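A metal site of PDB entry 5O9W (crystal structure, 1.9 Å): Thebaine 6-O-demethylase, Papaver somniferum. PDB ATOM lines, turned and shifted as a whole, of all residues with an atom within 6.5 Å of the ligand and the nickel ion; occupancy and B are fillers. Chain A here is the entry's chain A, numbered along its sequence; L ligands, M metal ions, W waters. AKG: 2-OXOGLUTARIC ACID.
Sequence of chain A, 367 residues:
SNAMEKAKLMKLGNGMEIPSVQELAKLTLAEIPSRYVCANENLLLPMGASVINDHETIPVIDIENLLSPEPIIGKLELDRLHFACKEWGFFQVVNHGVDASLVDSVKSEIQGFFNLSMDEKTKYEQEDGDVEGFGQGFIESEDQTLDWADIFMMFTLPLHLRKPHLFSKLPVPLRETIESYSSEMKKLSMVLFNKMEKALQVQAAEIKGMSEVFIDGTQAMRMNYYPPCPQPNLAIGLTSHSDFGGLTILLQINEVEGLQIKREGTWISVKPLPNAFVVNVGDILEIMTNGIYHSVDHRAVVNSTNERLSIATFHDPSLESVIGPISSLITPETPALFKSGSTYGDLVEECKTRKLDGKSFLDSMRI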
ATOM      1  N   PHE A  90      27.371  24.468   9.594  1.00  0.00           N
ATOM      2  CA  PHE A  90      27.311  23.741   8.331  1.00  0.00           C
ATOM      3  C   PHE A  90      27.709  24.732   7.250  1.00  0.00           C
ATOM      4  O   PHE A  90      27.313  25.904   7.332  1.00  0.00           O
ATOM      5  CB  PHE A  90      25.874  23.287   7.974  1.00  0.00           C
ATOM      6  CG  PHE A  90      25.566  21.889   8.388  1.00  0.00           C
ATOM      7  CD1 PHE A  90      25.231  21.610   9.721  1.00  0.00           C
ATOM      8  CD2 PHE A  90      25.610  20.839   7.470  1.00  0.00           C
ATOM      9  CE1 PHE A  90      24.969  20.311  10.125  1.00  0.00           C
ATOM     10  CE2 PHE A  90      25.331  19.547   7.852  1.00  0.00           C
ATOM     11  CZ  PHE A  90      25.025  19.274   9.193  1.00  0.00           C
ATOM     12  N   ARG A 222      31.038   6.587   6.496  1.00  0.00           N
ATOM     13  CA  ARG A 222      29.715   5.993   6.536  1.00  0.00           C
ATOM     14  C   ARG A 222      29.102   6.238   5.158  1.00  0.00           C
ATOM     15  O   ARG A 222      28.932   7.366   4.755  1.00  0.00           O
ATOM     16  CB  ARG A 222      28.877   6.640   7.620  1.00  0.00           C
ATOM     17  CG  ARG A 222      27.433   6.225   7.654  1.00  0.00           C
ATOM     18  CD  ARG A 222      26.706   6.867   8.836  1.00  0.00           C
ATOM     19  NE  ARG A 222      25.367   6.338   8.881  1.00  0.00           N
ATOM     20  CZ  ARG A 222      24.667   6.094   9.987  1.00  0.00           C
ATOM     21  NH1 ARG A 222      25.125   6.412  11.201  1.00  0.00           N
ATOM     22  NH2 ARG A 222      23.460   5.562   9.880  1.00  0.00           N
ATOM     23  N   ASN A 224      25.837   5.825   2.964  1.00  0.00           N
ATOM     24  CA  ASN A 224      24.416   5.758   3.252  1.00  0.00           C
ATOM     25  C   ASN A 224      23.651   5.471   1.975  1.00  0.00           C
ATOM     26  O   ASN A 224      23.825   6.200   0.974  1.00  0.00           O
ATOM     27  CB  ASN A 224      23.913   7.084   3.837  1.00  0.00           C
ATOM     28  CG  ASN A 224      24.613   7.467   5.120  1.00  0.00           C
ATOM     29  OD1 ASN A 224      24.470   6.787   6.159  1.00  0.00           O
ATOM     30  ND2 ASN A 224      25.368   8.596   5.078  1.00  0.00           N
ATOM     31  N   TYR A 226      19.746   5.217   0.757  1.00  0.00           N
ATOM     32  CA  TYR A 226      18.380   5.511   1.177  1.00  0.00           C
ATOM     33  C   TYR A 226      17.426   5.087   0.060  1.00  0.00           C
ATOM     34  O   TYR A 226      17.297   5.796  -0.941  1.00  0.00           O
ATOM     35  CB  TYR A 226      18.219   6.998   1.460  1.00  0.00           C
ATOM     36  CG  TYR A 226      19.168   7.600   2.467  1.00  0.00           C
ATOM     37  CD1 TYR A 226      18.972   7.435   3.826  1.00  0.00           C
ATOM     38  CD2 TYR A 226      20.266   8.357   2.065  1.00  0.00           C
ATOM     39  CE1 TYR A 226      19.820   8.001   4.768  1.00  0.00           C
ATOM     40  CE2 TYR A 226      21.101   8.948   2.998  1.00  0.00           C
ATOM     41  CZ  TYR A 226      20.873   8.753   4.343  1.00  0.00           C
ATOM     42  OH  TYR A 226      21.712   9.342   5.263  1.00  0.00           O
ATOM     43  N   LEU A 238      17.729   8.906   7.936  1.00  0.00           N
ATOM     44  CA  LEU A 238      18.659   8.911   9.033  1.00  0.00           C
ATOM     45  C   LEU A 238      18.081   9.806  10.142  1.00  0.00           C
ATOM     46  O   LEU A 238      17.927  11.021   9.948  1.00  0.00           O
ATOM     47  CB  LEU A 238      20.017   9.394   8.556  1.00  0.00           C
ATOM     48  CG  LEU A 238      21.152   9.460   9.604  1.00  0.00           C
ATOM     49  CD1 LEU A 238      21.423   8.123  10.246  1.00  0.00           C
ATOM     50  CD2 LEU A 238      22.421   9.980   8.932  1.00  0.00           C
ATOM     51  N   HIS A 241      20.232  13.780  14.489  1.00  0.00           N
ATOM     52  CA  HIS A 241      21.411  13.621  15.328  1.00  0.00           C
ATOM     53  C   HIS A 241      22.354  14.791  15.123  1.00  0.00           C
ATOM     54  O   HIS A 241      22.269  15.497  14.115  1.00  0.00           O
ATOM     55  CB  HIS A 241      22.153  12.314  14.964  1.00  0.00           C
ATOM     56  CG  HIS A 241      22.749  12.326  13.585  1.00  0.00           C
ATOM     57  ND1 HIS A 241      21.976  12.187  12.445  1.00  0.00           N
ATOM     58  CD2 HIS A 241      24.018  12.540  13.167  1.00  0.00           C
ATOM     59  CE1 HIS A 241      22.757  12.304  11.374  1.00  0.00           C
ATOM     60  NE2 HIS A 241      24.005  12.510  11.791  1.00  0.00           N
ATOM     61  N   SER A 242      23.256  14.991  16.068  1.00  0.00           N
ATOM     62  CA  SER A 242      24.451  15.795  15.810  1.00  0.00           C
ATOM     63  C   SER A 242      25.608  14.814  15.682  1.00  0.00           C
ATOM     64  O   SER A 242      25.601  13.739  16.326  1.00  0.00           O
ATOM     65  CB  SER A 242      24.678  16.854  16.885  1.00  0.00           C
ATOM     66  OG  SER A 242      24.919  16.291  18.160  1.00  0.00           O
ATOM     67  N   ASP A 243      26.566  15.126  14.808  1.00  0.00           N
ATOM     68  CA  ASP A 243      27.742  14.290  14.660  1.00  0.00           C
ATOM     69  C   ASP A 243      28.589  14.455  15.926  1.00  0.00           C
ATOM     70  O   ASP A 243      28.714  15.562  16.481  1.00  0.00           O
ATOM     71  CB  ASP A 243      28.552  14.637  13.397  1.00  0.00           C
ATOM     72  CG  ASP A 243      27.824  14.332  12.114  1.00  0.00           C
ATOM     73  OD1 ASP A 243      26.831  13.546  12.110  1.00  0.00           O
ATOM     74  OD2 ASP A 243      28.237  14.895  11.072  1.00  0.00           O
ATOM     75  N   THR A 248      32.947  16.704   9.862  1.00  0.00           N
ATOM     76  CA  THR A 248      32.376  15.787   8.881  1.00  0.00           C
ATOM     77  C   THR A 248      32.431  16.442   7.506  1.00  0.00           C
ATOM     78  O   THR A 248      32.068  17.599   7.374  1.00  0.00           O
ATOM     79  CB  THR A 248      30.939  15.473   9.217  1.00  0.00           C
ATOM     80  OG1 THR A 248      30.851  14.960  10.562  1.00  0.00           O
ATOM     81  CG2 THR A 248      30.366  14.429   8.258  1.00  0.00           C
ATOM     82  N   LEU A 250      30.873  15.647   3.834  1.00  0.00           N
ATOM     83  CA  LEU A 250      29.851  14.801   3.211  1.00  0.00           C
ATOM     84  C   LEU A 250      29.825  15.024   1.700  1.00  0.00           C
ATOM     85  O   LEU A 250      29.867  16.184   1.241  1.00  0.00           O
ATOM     86  CB  LEU A 250      28.480  15.179   3.773  1.00  0.00           C
ATOM     87  CG  LEU A 250      27.271  14.430   3.175  1.00  0.00           C
ATOM     88  CD1 LEU A 250      26.994  13.174   3.960  1.00  0.00           C
ATOM     89  CD2 LEU A 250      26.055  15.327   3.201  1.00  0.00           C
ATOM     90  N   GLN A 252      27.276  14.091  -1.400  1.00  0.00           N
ATOM     91  CA  GLN A 252      26.039  13.544  -1.900  1.00  0.00           C
ATOM     92  C   GLN A 252      26.362  12.912  -3.234  1.00  0.00           C
ATOM     93  O   GLN A 252      26.881  13.593  -4.179  1.00  0.00           O
ATOM     94  CB  GLN A 252      24.963  14.614  -2.004  1.00  0.00           C
ATOM     95  CG  GLN A 252      23.593  14.076  -2.384  1.00  0.00           C
ATOM     96  CD  GLN A 252      22.542  15.158  -2.330  1.00  0.00           C
ATOM     97  OE1 GLN A 252      22.030  15.475  -1.288  1.00  0.00           O
ATOM     98  NE2 GLN A 252      22.227  15.734  -3.474  1.00  0.00           N
ATOM     99  N   GLY A 258      17.848  15.459   0.286  1.00  0.00           N
ATOM    100  CA  GLY A 258      17.453  14.770   1.501  1.00  0.00           C
ATOM    101  C   GLY A 258      18.034  15.223   2.814  1.00  0.00           C
ATOM    102  O   GLY A 258      17.425  14.973   3.868  1.00  0.00           O
ATOM    103  N   LEU A 259      19.222  15.824   2.758  1.00  0.00           N
ATOM    104  CA  LEU A 259      19.828  16.372   3.956  1.00  0.00           C
ATOM    105  C   LEU A 259      19.041  17.601   4.457  1.00  0.00           C
ATOM    106  O   LEU A 259      18.779  18.533   3.674  1.00  0.00           O
ATOM    107  CB  LEU A 259      21.279  16.746   3.712  1.00  0.00           C
ATOM    108  CG  LEU A 259      22.018  17.459   4.848  1.00  0.00           C
ATOM    109  CD1 LEU A 259      22.104  16.546   6.069  1.00  0.00           C
ATOM    110  CD2 LEU A 259      23.376  17.872   4.385  1.00  0.00           C
ATOM    111  N   GLN A 260      18.705  17.603   5.737  1.00  0.00           N
ATOM    112  CA  GLN A 260      18.107  18.771   6.395  1.00  0.00           C
ATOM    113  C   GLN A 260      18.786  19.063   7.710  1.00  0.00           C
ATOM    114  O   GLN A 260      19.206  18.136   8.386  1.00  0.00           O
ATOM    115  CB  GLN A 260      16.613  18.553   6.641  1.00  0.00           C
ATOM    116  CG  GLN A 260      15.812  18.219   5.376  1.00  0.00           C
ATOM    117  CD  GLN A 260      14.336  17.979   5.647  1.00  0.00           C
ATOM    118  OE1 GLN A 260      13.915  17.775   6.786  1.00  0.00           O
ATOM    119  NE2 GLN A 260      13.549  17.937   4.559  1.00  0.00           N
ATOM    120  N   ASN A 280      30.420  19.924   8.284  1.00  0.00           N
ATOM    121  CA  ASN A 280      29.800  20.369   9.531  1.00  0.00           C
ATOM    122  C   ASN A 280      30.651  20.063  10.758  1.00  0.00           C
ATOM    123  O   ASN A 280      31.434  19.093  10.775  1.00  0.00           O
ATOM    124  CB  ASN A 280      28.379  19.807   9.737  1.00  0.00           C
ATOM    125  CG  ASN A 280      28.331  18.285   9.935  1.00  0.00           C
ATOM    126  OD1 ASN A 280      28.525  17.527   8.983  1.00  0.00           O
ATOM    127  ND2 ASN A 280      28.013  17.823  11.195  1.00  0.00           N
ATOM    128  N   HIS A 298      20.909  17.363  12.535  1.00  0.00           N
ATOM    129  CA  HIS A 298      20.542  17.170  11.139  1.00  0.00           C
ATOM    130  C   HIS A 298      19.966  15.763  10.920  1.00  0.00           C
ATOM    131  O   HIS A 298      20.087  14.868  11.756  1.00  0.00           O
ATOM    132  CB  HIS A 298      21.733  17.453  10.219  1.00  0.00           C
ATOM    133  CG  HIS A 298      22.949  16.654  10.554  1.00  0.00           C
ATOM    134  ND1 HIS A 298      23.761  16.946  11.634  1.00  0.00           N
ATOM    135  CD2 HIS A 298      23.466  15.546   9.986  1.00  0.00           C
ATOM    136  CE1 HIS A 298      24.726  16.056  11.698  1.00  0.00           C
ATOM    137  NE2 HIS A 298      24.583  15.190  10.706  1.00  0.00           N
ATOM    138  N   ARG A 299      19.268  15.614   9.822  1.00  0.00           N
ATOM    139  CA  ARG A 299      18.614  14.336   9.448  1.00  0.00           C
ATOM    140  C   ARG A 299      18.626  14.157   7.948  1.00  0.00           C
ATOM    141  O   ARG A 299      18.929  15.101   7.223  1.00  0.00           O
ATOM    142  CB  ARG A 299      17.174  14.322   9.976  1.00  0.00           C
ATOM    143  CG  ARG A 299      16.242  15.250   9.235  1.00  0.00           C
ATOM    144  CD  ARG A 299      14.883  15.349   9.914  1.00  0.00           C
ATOM    145  NE  ARG A 299      13.980  16.158   9.122  1.00  0.00           N
ATOM    146  CZ  ARG A 299      12.659  16.278   9.332  1.00  0.00           C
ATOM    147  NH1 ARG A 299      12.072  15.651  10.328  1.00  0.00           N
ATOM    148  NH2 ARG A 299      11.943  17.068   8.530  1.00  0.00           N
ATOM    149  N   ALA A 300      18.256  12.971   7.485  1.00  0.00           N
ATOM    150  CA  ALA A 300      18.095  12.736   6.067  1.00  0.00           C
ATOM    151  C   ALA A 300      16.727  12.157   5.854  1.00  0.00           C
ATOM    152  O   ALA A 300      16.319  11.178   6.491  1.00  0.00           O
ATOM    153  CB  ALA A 300      19.161  11.795   5.538  1.00  0.00           C
ATOM    154  N   ARG A 308      18.550   7.743  -2.716  1.00  0.00           N
ATOM    155  CA  ARG A 308      19.556   8.773  -2.458  1.00  0.00           C
ATOM    156  C   ARG A 308      20.773   8.057  -1.858  1.00  0.00           C
ATOM    157  O   ARG A 308      20.616   7.155  -1.046  1.00  0.00           O
ATOM    158  CB  ARG A 308      19.029   9.800  -1.470  1.00  0.00           C
ATOM    159  CG  ARG A 308      19.980  10.953  -1.185  1.00  0.00           C
ATOM    160  CD  ARG A 308      19.338  12.094  -0.431  1.00  0.00           C
ATOM    161  NE  ARG A 308      20.390  13.020  -0.078  1.00  0.00           N
ATOM    162  CZ  ARG A 308      21.107  12.981   1.054  1.00  0.00           C
ATOM    163  NH1 ARG A 308      22.105  13.832   1.176  1.00  0.00           N
ATOM    164  NH2 ARG A 308      20.823  12.157   2.059  1.00  0.00           N
ATOM    165  N   LEU A 309      21.964   8.429  -2.302  1.00  0.00           N
ATOM    166  CA  LEU A 309      23.215   7.941  -1.726  1.00  0.00           C
ATOM    167  C   LEU A 309      24.071   9.106  -1.202  1.00  0.00           C
ATOM    168  O   LEU A 309      24.096  10.181  -1.795  1.00  0.00           O
ATOM    169  CB  LEU A 309      24.017   7.133  -2.754  1.00  0.00           C
ATOM    170  CG  LEU A 309      23.444   5.752  -3.112  1.00  0.00           C
ATOM    171  CD1 LEU A 309      22.342   5.863  -4.144  1.00  0.00           C
ATOM    172  CD2 LEU A 309      24.541   4.816  -3.609  1.00  0.00           C
ATOM    173  N   SER A 310      24.831   8.853  -0.137  1.00  0.00           N
ATOM    174  CA  SER A 310      25.773   9.817   0.384  1.00  0.00           C
ATOM    175  C   SER A 310      26.929   9.076   1.066  1.00  0.00           C
ATOM    176  O   SER A 310      26.785   7.893   1.420  1.00  0.00           O
ATOM    177  CB  SER A 310      25.092  10.778   1.363  1.00  0.00           C
ATOM    178  OG  SER A 310      24.711  10.166   2.584  1.00  0.00           O
ATOM    179  N   ILE A 311      28.062   9.773   1.202  1.00  0.00           N
ATOM    180  CA  ILE A 311      29.184   9.255   1.983  1.00  0.00           C
ATOM    181  C   ILE A 311      29.679  10.386   2.891  1.00  0.00           C
ATOM    182  O   ILE A 311      30.055  11.462   2.438  1.00  0.00           O
ATOM    183  CB  ILE A 311      30.301   8.601   1.145  1.00  0.00           C
ATOM    184  CG1 ILE A 311      31.446   8.128   2.069  1.00  0.00           C
ATOM    185  CG2 ILE A 311      30.792   9.548   0.035  1.00  0.00           C
ATOM    186  CD1 ILE A 311      32.581   7.419   1.392  1.00  0.00           C
ATOM    187  N   ALA A 312      29.651  10.113   4.189  1.00  0.00           N
ATOM    188  CA  ALA A 312      30.117  11.030   5.204  1.00  0.00           C
ATOM    189  C   ALA A 312      31.507  10.542   5.668  1.00  0.00           C
ATOM    190  O   ALA A 312      31.657   9.372   6.026  1.00  0.00           O
ATOM    191  CB  ALA A 312      29.150  11.024   6.359  1.00  0.00           C
ATOM    192  N   PHE A 314      34.235  11.289   8.581  1.00  0.00           N
ATOM    193  CA  PHE A 314      34.339  11.894   9.889  1.00  0.00           C
ATOM    194  C   PHE A 314      35.790  12.015  10.290  1.00  0.00           C
ATOM    195  O   PHE A 314      36.553  11.063  10.147  1.00  0.00           O
ATOM    196  CB  PHE A 314      33.623  11.021  10.917  1.00  0.00           C
ATOM    197  CG  PHE A 314      32.222  10.736  10.571  1.00  0.00           C
ATOM    198  CD1 PHE A 314      31.231  11.690  10.767  1.00  0.00           C
ATOM    199  CD2 PHE A 314      31.864   9.510  10.021  1.00  0.00           C
ATOM    200  CE1 PHE A 314      29.919  11.445  10.412  1.00  0.00           C
ATOM    201  CE2 PHE A 314      30.551   9.260   9.675  1.00  0.00           C
ATOM    202  CZ  PHE A 314      29.583  10.234   9.852  1.00  0.00           C
HETATM  203  C1  AKG L   1      25.808  11.091   8.667  1.00  0.00           C
HETATM  204  O1  AKG L   1      26.138  11.424   9.835  1.00  0.00           O
HETATM  205  O2  AKG L   1      26.256  10.087   8.110  1.00  0.00           O
HETATM  206  C2  AKG L   1      24.828  11.940   7.963  1.00  0.00           C
HETATM  207  O5  AKG L   1      24.291  12.848   8.599  1.00  0.00           O
HETATM  208  C3  AKG L   1      24.519  11.737   6.520  1.00  0.00           C
HETATM  209  C4  AKG L   1      23.545  12.785   5.977  1.00  0.00           C
HETATM  210  C5  AKG L   1      23.151  12.533   4.537  1.00  0.00           C
HETATM  211  O3  AKG L   1      23.040  11.334   4.141  1.00  0.00           O
HETATM  212  O4  AKG L   1      22.975  13.540   3.807  1.00  0.00           O
HETATM  213 NI    NI M   1      25.457  13.284  10.428  1.00  0.00          NI
HETATM  214  O   HOH W   1      25.925   9.140  11.673  1.00  0.00           O
HETATM  215  O   HOH W   2      26.875  14.075   9.097  1.00  0.00           O
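O of Ala 312 is in hydrogen-bond range of N of Arg 222 (2.9 Å).
N of Tyr 226 is in hydrogen-bond range of O of Arg 308, at 2.8 Å.
NE of Arg 222 is in hydrogen-bond range of OD1 of Asn 224, 2.9 Å away.
The side-chain amide oxygen (OE1) of Gln 252 lies within hydrogen-bond range of the guanidinium group (NH1) of Arg 308, 3.0 Å away.
The side-chain carboxylate (OD2) of Asp 243 lies within hydrogen-bond range of the side-chain hydroxyl (OG1) of Thr 248, at 2.7 Å.
The side-chain carboxylate (OD2) of Asp 243 lies within hydrogen-bond range of the side-chain amide nitrogen (ND2) of Asn 280 (2.9 Å).
The backbone carbonyl oxygen (O) of Ser 310 lies within hydrogen-bond range of the backbone NH (N) of Asn 224, at 2.7 Å.
The backbone NH (N) of Leu 238 lies within hydrogen-bond range of the backbone carbonyl oxygen (O) of Ala 300 (3.0 Å).
CD2 of Leu 238 touches C2 of the ligand, at 3.3 Å.
Leu 250 touches the ligand (CD2 to O4, 3.6 Å).
Leu 259 touches the ligand (CB to O4, 3.6 Å).
Ala 312 touches the ligand (CB to O2, 3.5 Å).
CZ of Phe 314 touches O1 of the ligand (3.6 Å).
Hydrophobic or aromatic side chains within 4 Å of the ligand: Tyr 226, Leu 238, His 241, Leu 250, Leu 259, His 298, Ala 312 and Phe 314.
13 residues have an atom within 4 Å of the ligand: Arg 222, Asn 224, Tyr 226, Leu 238, His 241, Asp 243, Leu 250, Leu 259, His 298, Arg 308, Ser 310, Ala 312 and Phe 314.
The guanidinium group (NE) of Arg 222 is in salt-bridge range of an oxygen (O2) of the ligand (3.9 Å).
An oxygen (O3) of the ligand lies within hydrogen-bond range of the side-chain hydroxyl of Ser 310, at 2.6 Å.
The guanidinium group of Arg 308 lies within salt-bridge range of an oxygen (O4) of the ligand (2.8 Å).
ND2 of Asn 224 lies within hydrogen-bond range of O2 of the ligand, at 3.5 Å.
O3 of the ligand lies within hydrogen-bond range of OH of Tyr 226.
Of the 24 residues printed, 3 come within 4 Å of the nickel ion.
Along chain A the residues within 4 Å of the nickel ion span positions 241 to 298.
The nearest printed residue that does not touch the nickel ion is Leu 238 (4.7 Å).
The nickel ion is bound by an oxygen (O1) of the ligand (2.1 Å), water W2 (2.1 Å), a ring nitrogen (NE2) of His 298 (2.1 Å), a ring nitrogen (NE2) of His 241 (2.1 Å), the side-chain carboxylate of Asp 243 (2.2 Å) and an oxygen (O5) of the ligand (2.2 Å).
The nickel ion has six donor atoms within binding distance.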
